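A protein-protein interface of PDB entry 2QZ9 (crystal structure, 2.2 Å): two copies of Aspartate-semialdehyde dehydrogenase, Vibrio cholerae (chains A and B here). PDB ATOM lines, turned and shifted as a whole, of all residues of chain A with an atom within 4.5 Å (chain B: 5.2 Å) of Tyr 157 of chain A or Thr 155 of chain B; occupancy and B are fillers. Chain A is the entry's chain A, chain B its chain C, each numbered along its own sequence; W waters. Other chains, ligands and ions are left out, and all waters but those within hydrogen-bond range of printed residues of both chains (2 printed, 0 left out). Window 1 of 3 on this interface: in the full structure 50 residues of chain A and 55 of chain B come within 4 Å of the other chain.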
ATOM      1  N   THR A 155     -20.569   0.091  -3.028  1.00  0.00           N
ATOM      2  CA  THR A 155     -21.632   0.436  -3.960  1.00  0.00           C
ATOM      3  C   THR A 155     -22.460   1.510  -3.286  1.00  0.00           C
ATOM      4  O   THR A 155     -22.652   1.484  -2.072  1.00  0.00           O
ATOM      5  CB  THR A 155     -22.518  -0.772  -4.364  1.00  0.00           C
ATOM      6  OG1 THR A 155     -23.340  -1.170  -3.249  1.00  0.00           O
ATOM      7  CG2 THR A 155     -21.652  -1.956  -4.809  1.00  0.00           C
ATOM      8  N   THR A 156     -22.938   2.456  -4.075  1.00  0.00           N
ATOM      9  CA  THR A 156     -23.532   3.643  -3.516  1.00  0.00           C
ATOM     10  C   THR A 156     -24.995   3.763  -3.894  1.00  0.00           C
ATOM     11  O   THR A 156     -25.463   3.151  -4.850  1.00  0.00           O
ATOM     12  CB  THR A 156     -22.771   4.921  -3.950  1.00  0.00           C
ATOM     13  OG1 THR A 156     -23.066   5.195  -5.324  1.00  0.00           O
ATOM     14  CG2 THR A 156     -21.260   4.737  -3.774  1.00  0.00           C
ATOM     15  N   TYR A 157     -25.707   4.532  -3.084  1.00  0.00           N
ATOM     16  CA  TYR A 157     -27.128   4.739  -3.234  1.00  0.00           C
ATOM     17  C   TYR A 157     -27.233   6.258  -3.159  1.00  0.00           C
ATOM     18  O   TYR A 157     -27.456   6.820  -2.087  1.00  0.00           O
ATOM     19  CB  TYR A 157     -27.871   4.019  -2.091  1.00  0.00           C
ATOM     20  CG  TYR A 157     -27.686   2.507  -2.130  1.00  0.00           C
ATOM     21  CD1 TYR A 157     -26.459   1.914  -1.790  1.00  0.00           C
ATOM     22  CD2 TYR A 157     -28.731   1.669  -2.526  1.00  0.00           C
ATOM     23  CE1 TYR A 157     -26.282   0.534  -1.856  1.00  0.00           C
ATOM     24  CE2 TYR A 157     -28.562   0.285  -2.576  1.00  0.00           C
ATOM     25  CZ  TYR A 157     -27.334  -0.266  -2.245  1.00  0.00           C
ATOM     26  OH  TYR A 157     -27.173  -1.617  -2.317  1.00  0.00           O
ATOM     27  N   GLN A 158     -27.009   6.908  -4.302  1.00  0.00           N
ATOM     28  CA  GLN A 158     -26.803   8.361  -4.339  1.00  0.00           C
ATOM     29  C   GLN A 158     -28.035   9.166  -4.751  1.00  0.00           C
ATOM     30  O   GLN A 158     -28.670   8.885  -5.763  1.00  0.00           O
ATOM     31  CB  GLN A 158     -25.595   8.719  -5.240  1.00  0.00           C
ATOM     32  CG  GLN A 158     -24.256   8.375  -4.571  1.00  0.00           C
ATOM     33  CD  GLN A 158     -23.041   8.651  -5.445  1.00  0.00           C
ATOM     34  OE1 GLN A 158     -22.417   7.724  -5.972  1.00  0.00           O
ATOM     35  NE2 GLN A 158     -22.691   9.925  -5.592  1.00  0.00           N
ATOM     36  N   SER A 159     -28.354  10.177  -3.956  1.00  0.00           N
ATOM     37  CA  SER A 159     -29.542  10.996  -4.179  1.00  0.00           C
ATOM     38  C   SER A 159     -29.381  11.945  -5.366  1.00  0.00           C
ATOM     39  O   SER A 159     -28.244  12.286  -5.769  1.00  0.00           O
ATOM     40  CB  SER A 159     -29.883  11.779  -2.922  1.00  0.00           C
ATOM     41  OG  SER A 159     -28.827  12.654  -2.581  1.00  0.00           O
ATOM     42  N   VAL A 236     -24.414   4.332  -8.035  1.00  0.00           N
ATOM     43  CA  VAL A 236     -25.790   4.231  -8.544  1.00  0.00           C
ATOM     44  C   VAL A 236     -26.641   5.426  -8.081  1.00  0.00           C
ATOM     45  O   VAL A 236     -26.631   5.772  -6.905  1.00  0.00           O
ATOM     46  CB  VAL A 236     -26.473   2.896  -8.087  1.00  0.00           C
ATOM     47  CG1 VAL A 236     -27.880   2.755  -8.676  1.00  0.00           C
ATOM     48  CG2 VAL A 236     -25.607   1.652  -8.451  1.00  0.00           C
ATOM     49  N   VAL A 238     -30.159   6.813  -7.052  1.00  0.00           N
ATOM     50  CA  VAL A 238     -31.434   6.285  -6.549  1.00  0.00           C
ATOM     51  C   VAL A 238     -32.478   7.413  -6.377  1.00  0.00           C
ATOM     52  O   VAL A 238     -32.093   8.585  -6.318  1.00  0.00           O
ATOM     53  CB  VAL A 238     -31.246   5.459  -5.237  1.00  0.00           C
ATOM     54  CG1 VAL A 238     -30.424   4.198  -5.522  1.00  0.00           C
ATOM     55  CG2 VAL A 238     -30.604   6.308  -4.126  1.00  0.00           C
ATOM     56  N   GLY A 243     -29.107  13.219   0.865  1.00  0.00           N
ATOM     57  CA  GLY A 243     -28.318  12.178   1.532  1.00  0.00           C
ATOM     58  C   GLY A 243     -27.785  11.113   0.579  1.00  0.00           C
ATOM     59  O   GLY A 243     -28.460  10.715  -0.361  1.00  0.00           O
ATOM     60  N   HIS A 244     -26.563  10.644   0.821  1.00  0.00           N
ATOM     61  CA  HIS A 244     -26.055   9.473   0.106  1.00  0.00           C
ATOM     62  C   HIS A 244     -25.850   8.357   1.100  1.00  0.00           C
ATOM     63  O   HIS A 244     -25.538   8.606   2.249  1.00  0.00           O
ATOM     64  CB  HIS A 244     -24.729   9.752  -0.603  1.00  0.00           C
ATOM     65  CG  HIS A 244     -24.828  10.756  -1.704  1.00  0.00           C
ATOM     66  ND1 HIS A 244     -23.728  11.436  -2.189  1.00  0.00           N
ATOM     67  CD2 HIS A 244     -25.888  11.201  -2.411  1.00  0.00           C
ATOM     68  CE1 HIS A 244     -24.110  12.246  -3.160  1.00  0.00           C
ATOM     69  NE2 HIS A 244     -25.416  12.127  -3.310  1.00  0.00           N
ATOM     70  N   ALA A 245     -26.031   7.127   0.637  1.00  0.00           N
ATOM     71  CA  ALA A 245     -25.759   5.950   1.437  1.00  0.00           C
ATOM     72  C   ALA A 245     -24.763   5.080   0.679  1.00  0.00           C
ATOM     73  O   ALA A 245     -24.725   5.104  -0.547  1.00  0.00           O
ATOM     74  CB  ALA A 245     -27.046   5.191   1.695  1.00  0.00           C
ATOM     75  N   ALA A 247     -22.876   1.058   0.748  1.00  0.00           N
ATOM     76  CA  ALA A 247     -22.595  -0.257   1.247  1.00  0.00           C
ATOM     77  C   ALA A 247     -21.093  -0.515   1.107  1.00  0.00           C
ATOM     78  O   ALA A 247     -20.581  -0.615  -0.013  1.00  0.00           O
ATOM     79  CB  ALA A 247     -23.374  -1.237   0.412  1.00  0.00           C
ATOM     80  N   HIS A 249     -17.750  -2.813   1.911  1.00  0.00           N
ATOM     81  CA  HIS A 249     -17.255  -4.145   2.257  1.00  0.00           C
ATOM     82  C   HIS A 249     -15.711  -4.094   2.211  1.00  0.00           C
ATOM     83  O   HIS A 249     -15.097  -4.109   1.129  1.00  0.00           O
ATOM     84  CB  HIS A 249     -17.767  -5.201   1.254  1.00  0.00           C
ATOM     85  CG  HIS A 249     -19.263  -5.381   1.228  1.00  0.00           C
ATOM     86  ND1 HIS A 249     -19.879  -6.297   0.398  1.00  0.00           N
ATOM     87  CD2 HIS A 249     -20.260  -4.787   1.933  1.00  0.00           C
ATOM     88  CE1 HIS A 249     -21.184  -6.262   0.593  1.00  0.00           C
ATOM     89  NE2 HIS A 249     -21.442  -5.349   1.514  1.00  0.00           N
ATOM     90  N   GLN A 282     -31.244   7.635   4.693  1.00  0.00           N
ATOM     91  CA  GLN A 282     -31.266   8.974   4.111  1.00  0.00           C
ATOM     92  C   GLN A 282     -32.443   9.864   4.582  1.00  0.00           C
ATOM     93  O   GLN A 282     -32.213  10.914   5.175  1.00  0.00           O
ATOM     94  CB  GLN A 282     -31.238   8.857   2.584  1.00  0.00           C
ATOM     95  CG  GLN A 282     -29.890   8.350   2.029  1.00  0.00           C
ATOM     96  CD  GLN A 282     -30.047   7.499   0.786  1.00  0.00           C
ATOM     97  OE1 GLN A 282     -30.718   6.462   0.812  1.00  0.00           O
ATOM     98  NE2 GLN A 282     -29.427   7.924  -0.311  1.00  0.00           N
ATOM     99  N   TRP A 310     -22.620   0.070   6.641  1.00  0.00           N
ATOM    100  CA  TRP A 310     -23.551   0.891   5.861  1.00  0.00           C
ATOM    101  C   TRP A 310     -23.269   2.332   6.264  1.00  0.00           C
ATOM    102  O   TRP A 310     -23.239   2.642   7.441  1.00  0.00           O
ATOM    103  CB  TRP A 310     -24.998   0.480   6.181  1.00  0.00           C
ATOM    104  CG  TRP A 310     -26.143   1.311   5.577  1.00  0.00           C
ATOM    105  CD1 TRP A 310     -26.968   2.179   6.263  1.00  0.00           C
ATOM    106  CD2 TRP A 310     -26.626   1.298   4.219  1.00  0.00           C
ATOM    107  NE1 TRP A 310     -27.901   2.718   5.413  1.00  0.00           N
ATOM    108  CE2 TRP A 310     -27.730   2.191   4.161  1.00  0.00           C
ATOM    109  CE3 TRP A 310     -26.230   0.631   3.045  1.00  0.00           C
ATOM    110  CZ2 TRP A 310     -28.422   2.456   2.976  1.00  0.00           C
ATOM    111  CZ3 TRP A 310     -26.925   0.883   1.875  1.00  0.00           C
ATOM    112  CH2 TRP A 310     -28.022   1.787   1.849  1.00  0.00           C
ATOM    113  N   ASN B 153     -18.754 -10.357  -3.993  1.00  0.00           N
ATOM    114  CA  ASN B 153     -19.368  -9.252  -3.261  1.00  0.00           C
ATOM    115  C   ASN B 153     -20.610  -8.802  -4.033  1.00  0.00           C
ATOM    116  O   ASN B 153     -20.551  -8.561  -5.243  1.00  0.00           O
ATOM    117  CB  ASN B 153     -18.406  -8.075  -3.074  1.00  0.00           C
ATOM    118  CG  ASN B 153     -17.449  -8.275  -1.919  1.00  0.00           C
ATOM    119  OD1 ASN B 153     -16.290  -8.642  -2.127  1.00  0.00           O
ATOM    120  ND2 ASN B 153     -17.922  -8.041  -0.695  1.00  0.00           N
ATOM    121  N   VAL B 154     -21.736  -8.719  -3.347  1.00  0.00           N
ATOM    122  CA  VAL B 154     -22.967  -8.305  -4.006  1.00  0.00           C
ATOM    123  C   VAL B 154     -23.744  -7.361  -3.091  1.00  0.00           C
ATOM    124  O   VAL B 154     -23.826  -7.580  -1.888  1.00  0.00           O
ATOM    125  CB  VAL B 154     -23.819  -9.545  -4.482  1.00  0.00           C
ATOM    126  CG1 VAL B 154     -24.180 -10.475  -3.317  1.00  0.00           C
ATOM    127  CG2 VAL B 154     -25.083  -9.130  -5.285  1.00  0.00           C
ATOM    128  N   THR B 155     -24.279  -6.289  -3.664  1.00  0.00           N
ATOM    129  CA  THR B 155     -25.249  -5.471  -2.964  1.00  0.00           C
ATOM    130  C   THR B 155     -26.439  -5.297  -3.885  1.00  0.00           C
ATOM    131  O   THR B 155     -26.277  -5.161  -5.102  1.00  0.00           O
ATOM    132  CB  THR B 155     -24.708  -4.092  -2.551  1.00  0.00           C
ATOM    133  OG1 THR B 155     -24.490  -3.313  -3.729  1.00  0.00           O
ATOM    134  CG2 THR B 155     -23.409  -4.212  -1.755  1.00  0.00           C
ATOM    135  N   THR B 156     -27.635  -5.295  -3.305  1.00  0.00           N
ATOM    136  CA  THR B 156     -28.840  -5.343  -4.107  1.00  0.00           C
ATOM    137  C   THR B 156     -29.606  -4.028  -4.078  1.00  0.00           C
ATOM    138  O   THR B 156     -29.422  -3.210  -3.188  1.00  0.00           O
ATOM    139  CB  THR B 156     -29.776  -6.488  -3.673  1.00  0.00           C
ATOM    140  OG1 THR B 156     -30.274  -6.206  -2.362  1.00  0.00           O
ATOM    141  CG2 THR B 156     -29.044  -7.808  -3.685  1.00  0.00           C
ATOM    142  N   TYR B 157     -30.436  -3.840  -5.098  1.00  0.00           N
ATOM    143  CA  TYR B 157     -31.331  -2.710  -5.217  1.00  0.00           C
ATOM    144  C   TYR B 157     -32.698  -3.364  -5.434  1.00  0.00           C
ATOM    145  O   TYR B 157     -33.069  -3.636  -6.560  1.00  0.00           O
ATOM    146  CB  TYR B 157     -30.866  -1.859  -6.418  1.00  0.00           C
ATOM    147  CG  TYR B 157     -29.489  -1.282  -6.179  1.00  0.00           C
ATOM    148  CD1 TYR B 157     -28.353  -2.097  -6.172  1.00  0.00           C
ATOM    149  CD2 TYR B 157     -29.328   0.070  -5.912  1.00  0.00           C
ATOM    150  CE1 TYR B 157     -27.085  -1.565  -5.923  1.00  0.00           C
ATOM    151  CE2 TYR B 157     -28.066   0.617  -5.676  1.00  0.00           C
ATOM    152  CZ  TYR B 157     -26.957  -0.208  -5.675  1.00  0.00           C
ATOM    153  OH  TYR B 157     -25.724   0.337  -5.404  1.00  0.00           O
ATOM    154  N   CYS B 197     -33.908   4.540   1.043  1.00  0.00           N
ATOM    155  CA  CYS B 197     -33.302   3.224   0.857  1.00  0.00           C
ATOM    156  C   CYS B 197     -33.148   2.609   2.234  1.00  0.00           C
ATOM    157  O   CYS B 197     -32.715   3.277   3.169  1.00  0.00           O
ATOM    158  CB  CYS B 197     -31.936   3.329   0.165  1.00  0.00           C
ATOM    159  SG  CYS B 197     -31.980   4.015  -1.492  1.00  0.00           S
ATOM    160  N   THR B 234     -24.906  -7.333   0.813  1.00  0.00           N
ATOM    161  CA  THR B 234     -25.737  -6.375   1.542  1.00  0.00           C
ATOM    162  C   THR B 234     -27.013  -6.193   0.732  1.00  0.00           C
ATOM    163  O   THR B 234     -26.961  -5.766  -0.427  1.00  0.00           O
ATOM    164  CB  THR B 234     -25.068  -4.981   1.761  1.00  0.00           C
ATOM    165  OG1 THR B 234     -23.921  -5.097   2.618  1.00  0.00           O
ATOM    166  CG2 THR B 234     -26.048  -4.001   2.424  1.00  0.00           C
ATOM    167  N   VAL B 236     -30.561  -4.316   0.129  1.00  0.00           N
ATOM    168  CA  VAL B 236     -31.143  -3.008   0.360  1.00  0.00           C
ATOM    169  C   VAL B 236     -32.486  -2.876  -0.379  1.00  0.00           C
ATOM    170  O   VAL B 236     -32.581  -3.185  -1.562  1.00  0.00           O
ATOM    171  CB  VAL B 236     -30.182  -1.877  -0.104  1.00  0.00           C
ATOM    172  CG1 VAL B 236     -30.752  -0.497   0.218  1.00  0.00           C
ATOM    173  CG2 VAL B 236     -28.785  -2.044   0.551  1.00  0.00           C
ATOM    174  N   VAL B 238     -35.204  -0.564  -2.125  1.00  0.00           N
ATOM    175  CA  VAL B 238     -35.228   0.725  -2.842  1.00  0.00           C
ATOM    176  C   VAL B 238     -36.661   1.111  -3.296  1.00  0.00           C
ATOM    177  O   VAL B 238     -37.528   0.240  -3.383  1.00  0.00           O
ATOM    178  CB  VAL B 238     -34.229   0.760  -4.058  1.00  0.00           C
ATOM    179  CG1 VAL B 238     -32.782   0.721  -3.570  1.00  0.00           C
ATOM    180  CG2 VAL B 238     -34.508  -0.344  -5.037  1.00  0.00           C
ATOM    181  N   ALA B 245     -32.305  -5.150  -8.978  1.00  0.00           N
ATOM    182  CA  ALA B 245     -30.969  -4.985  -9.524  1.00  0.00           C
ATOM    183  C   ALA B 245     -29.890  -5.360  -8.506  1.00  0.00           C
ATOM    184  O   ALA B 245     -30.086  -5.277  -7.300  1.00  0.00           O
ATOM    185  CB  ALA B 245     -30.768  -3.567 -10.050  1.00  0.00           C
ATOM    186  N   GLU B 246     -28.743  -5.771  -9.016  1.00  0.00           N
ATOM    187  CA  GLU B 246     -27.638  -6.136  -8.168  1.00  0.00           C
ATOM    188  C   GLU B 246     -26.350  -5.606  -8.741  1.00  0.00           C
ATOM    189  O   GLU B 246     -26.088  -5.721  -9.944  1.00  0.00           O
ATOM    190  CB  GLU B 246     -27.546  -7.651  -8.027  1.00  0.00           C
ATOM    191  CG  GLU B 246     -28.832  -8.266  -7.544  1.00  0.00           C
ATOM    192  CD  GLU B 246     -28.863  -9.764  -7.697  1.00  0.00           C
ATOM    193  OE1 GLU B 246     -28.114 -10.293  -8.545  1.00  0.00           O
ATOM    194  OE2 GLU B 246     -29.667 -10.394  -6.978  1.00  0.00           O
ATOM    195  N   ALA B 247     -25.556  -5.032  -7.848  1.00  0.00           N
ATOM    196  CA  ALA B 247     -24.174  -4.705  -8.128  1.00  0.00           C
ATOM    197  C   ALA B 247     -23.306  -5.900  -7.698  1.00  0.00           C
ATOM    198  O   ALA B 247     -23.222  -6.212  -6.508  1.00  0.00           O
ATOM    199  CB  ALA B 247     -23.825  -3.466  -7.339  1.00  0.00           C
HETATM  200  O   HOH W   1     -14.264  -6.814  -0.047  1.00  0.00           O
HETATM  201  O   HOH W   2     -30.803   5.324   2.999  1.00  0.00           O
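The side-chain hydroxyl (OG1) of Thr 155 of chain B sits at hydrogen-bond distance from the side-chain hydroxyl (OG1) of Thr 155 of chain A (2.5 Å). The backbone carbonyl oxygen (O) of Thr 156 of chain A sits at hydrogen-bond distance from the side-chain hydroxyl (OH) of Tyr 157 of chain B, 2.9 Å away. OH of Tyr 157 of chain A lies within hydrogen-bond range of OG1 of Thr 155 of chain B (3.5 Å). The side-chain hydroxyl of Tyr 157 of chain A is in hydrogen-bond range of the backbone carbonyl oxygen of Thr 156 of chain B (2.9 Å). ND1 of His 249 of chain A sits at hydrogen-bond distance from ND2 of Asn 153 of chain B (2.8 Å). A ring nitrogen (NE2) of His 249 of chain A is in hydrogen-bond range of the side-chain hydroxyl (OG1) of Thr 234 of chain B (2.7 Å). The side-chain amide oxygen (OE1) of Gln 282 of chain A sits close to the side-chain sulfur (SG) of Cys 197 of chain B.
The backbone NH of Tyr 157 of chain A is in hydrogen-bond range of the backbone carbonyl oxygen of Ala 245 of chain A (2.8 Å). N of Gln 158 of chain A sits at hydrogen-bond distance from O of Val 236 of chain A (2.9 Å). The side-chain amide nitrogen of Gln 282 of chain A sits at hydrogen-bond distance from the backbone carbonyl oxygen of Gly 243 of chain A, 3.0 Å away. N of Thr 234 of chain B lies within hydrogen-bond range of O of Val 154 of chain B, at 2.9 Å. The backbone carbonyl oxygen (O) of Thr 155 of chain B is in hydrogen-bond range of the backbone NH (N) of Ala 247 of chain B, 2.8 Å away. The backbone NH (N) of Tyr 157 of chain B lies within hydrogen-bond range of the backbone carbonyl oxygen (O) of Ala 245 of chain B (2.7 Å).
CB of Thr 155 of chain A touches OH of Tyr 157 of chain B, 3.5 Å away. CG2 of Thr 155 of chain A touches CB of Ala 247 of chain B, at 3.7 Å. Tyr 157 of chain B touches Tyr 157 of chain A. Val 236 of chain B touches Tyr 157 of chain A. Val 236 of chain A touches Tyr 157 of chain B (CG2 to OH, 3.3 Å). SG of Cys 197 of chain B touches CG2 of Val 238 of chain A, at 3.8 Å. Thr 155 of chain B touches Ala 247 of chain A. His 249 of chain A touches Val 154 of chain B (CE1 to O, 3.9 Å). CE1 of His 249 of chain A touches CG2 of Thr 155 of chain B, 3.8 Å away. Val 236 of chain B touches Trp 310 of chain A.
Tyr 157 of chain A touches just these residues of chain B: Thr 155, Thr 156, Tyr 157 and Val 236. Printed residues of chain B within 4 Å of Val 236 of chain A: Tyr 157. Gly 243 of chain A touches none of the printed residues of chain B. Printed residues of chain B within 4 Å of Ala 247 of chain A: Thr 155 (3.7 Å). Of the printed residues of chain B, His 249 of chain A touches Asn 153 (2.8 Å), Val 154 (3.9 Å), Thr 155 (3.8 Å) and Thr 234 (2.7 Å). Of the printed residues of chain A, Val 154 of chain B touches His 249.
Of the 12 printed residues of chain B, 9 touch a printed residue of chain A. Hydrophobic or aromatic side chains of chain B within 4 Å of the printed part of chain A: Tyr 157, Val 236 and Ala 247. Along chain A the printed residues that touch a printed residue of chain B span positions 155 to 310. Among the printed residues, 17 pairs touch across the chains.
Thr 155 of chain A touches its own counterpart, Thr 155 of chain B. Thr 155 of chain A touches Ala 247 of chain B, and with the chains exchanged Ala 247 of chain A touches Thr 155 of chain B. Thr 156 of chain A touches Tyr 157 of chain B, and with the chains exchanged Tyr 157 of chain A touches Thr 156 of chain B. Tyr 157 of chain A touches Val 236 of chain B, and with the chains exchanged Val 236 of chain A touches Tyr 157 of chain B. 7 positions are printed for both chains.
Water W2 lies within hydrogen-bond range of OE1 of Gln 282 of chain A and O of Cys 197 of chain B. Water W1 lies within hydrogen-bond range of O of His 249 of chain A (3.1 Å) and OD1 of Asn 153 of chain B (3.4 Å).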
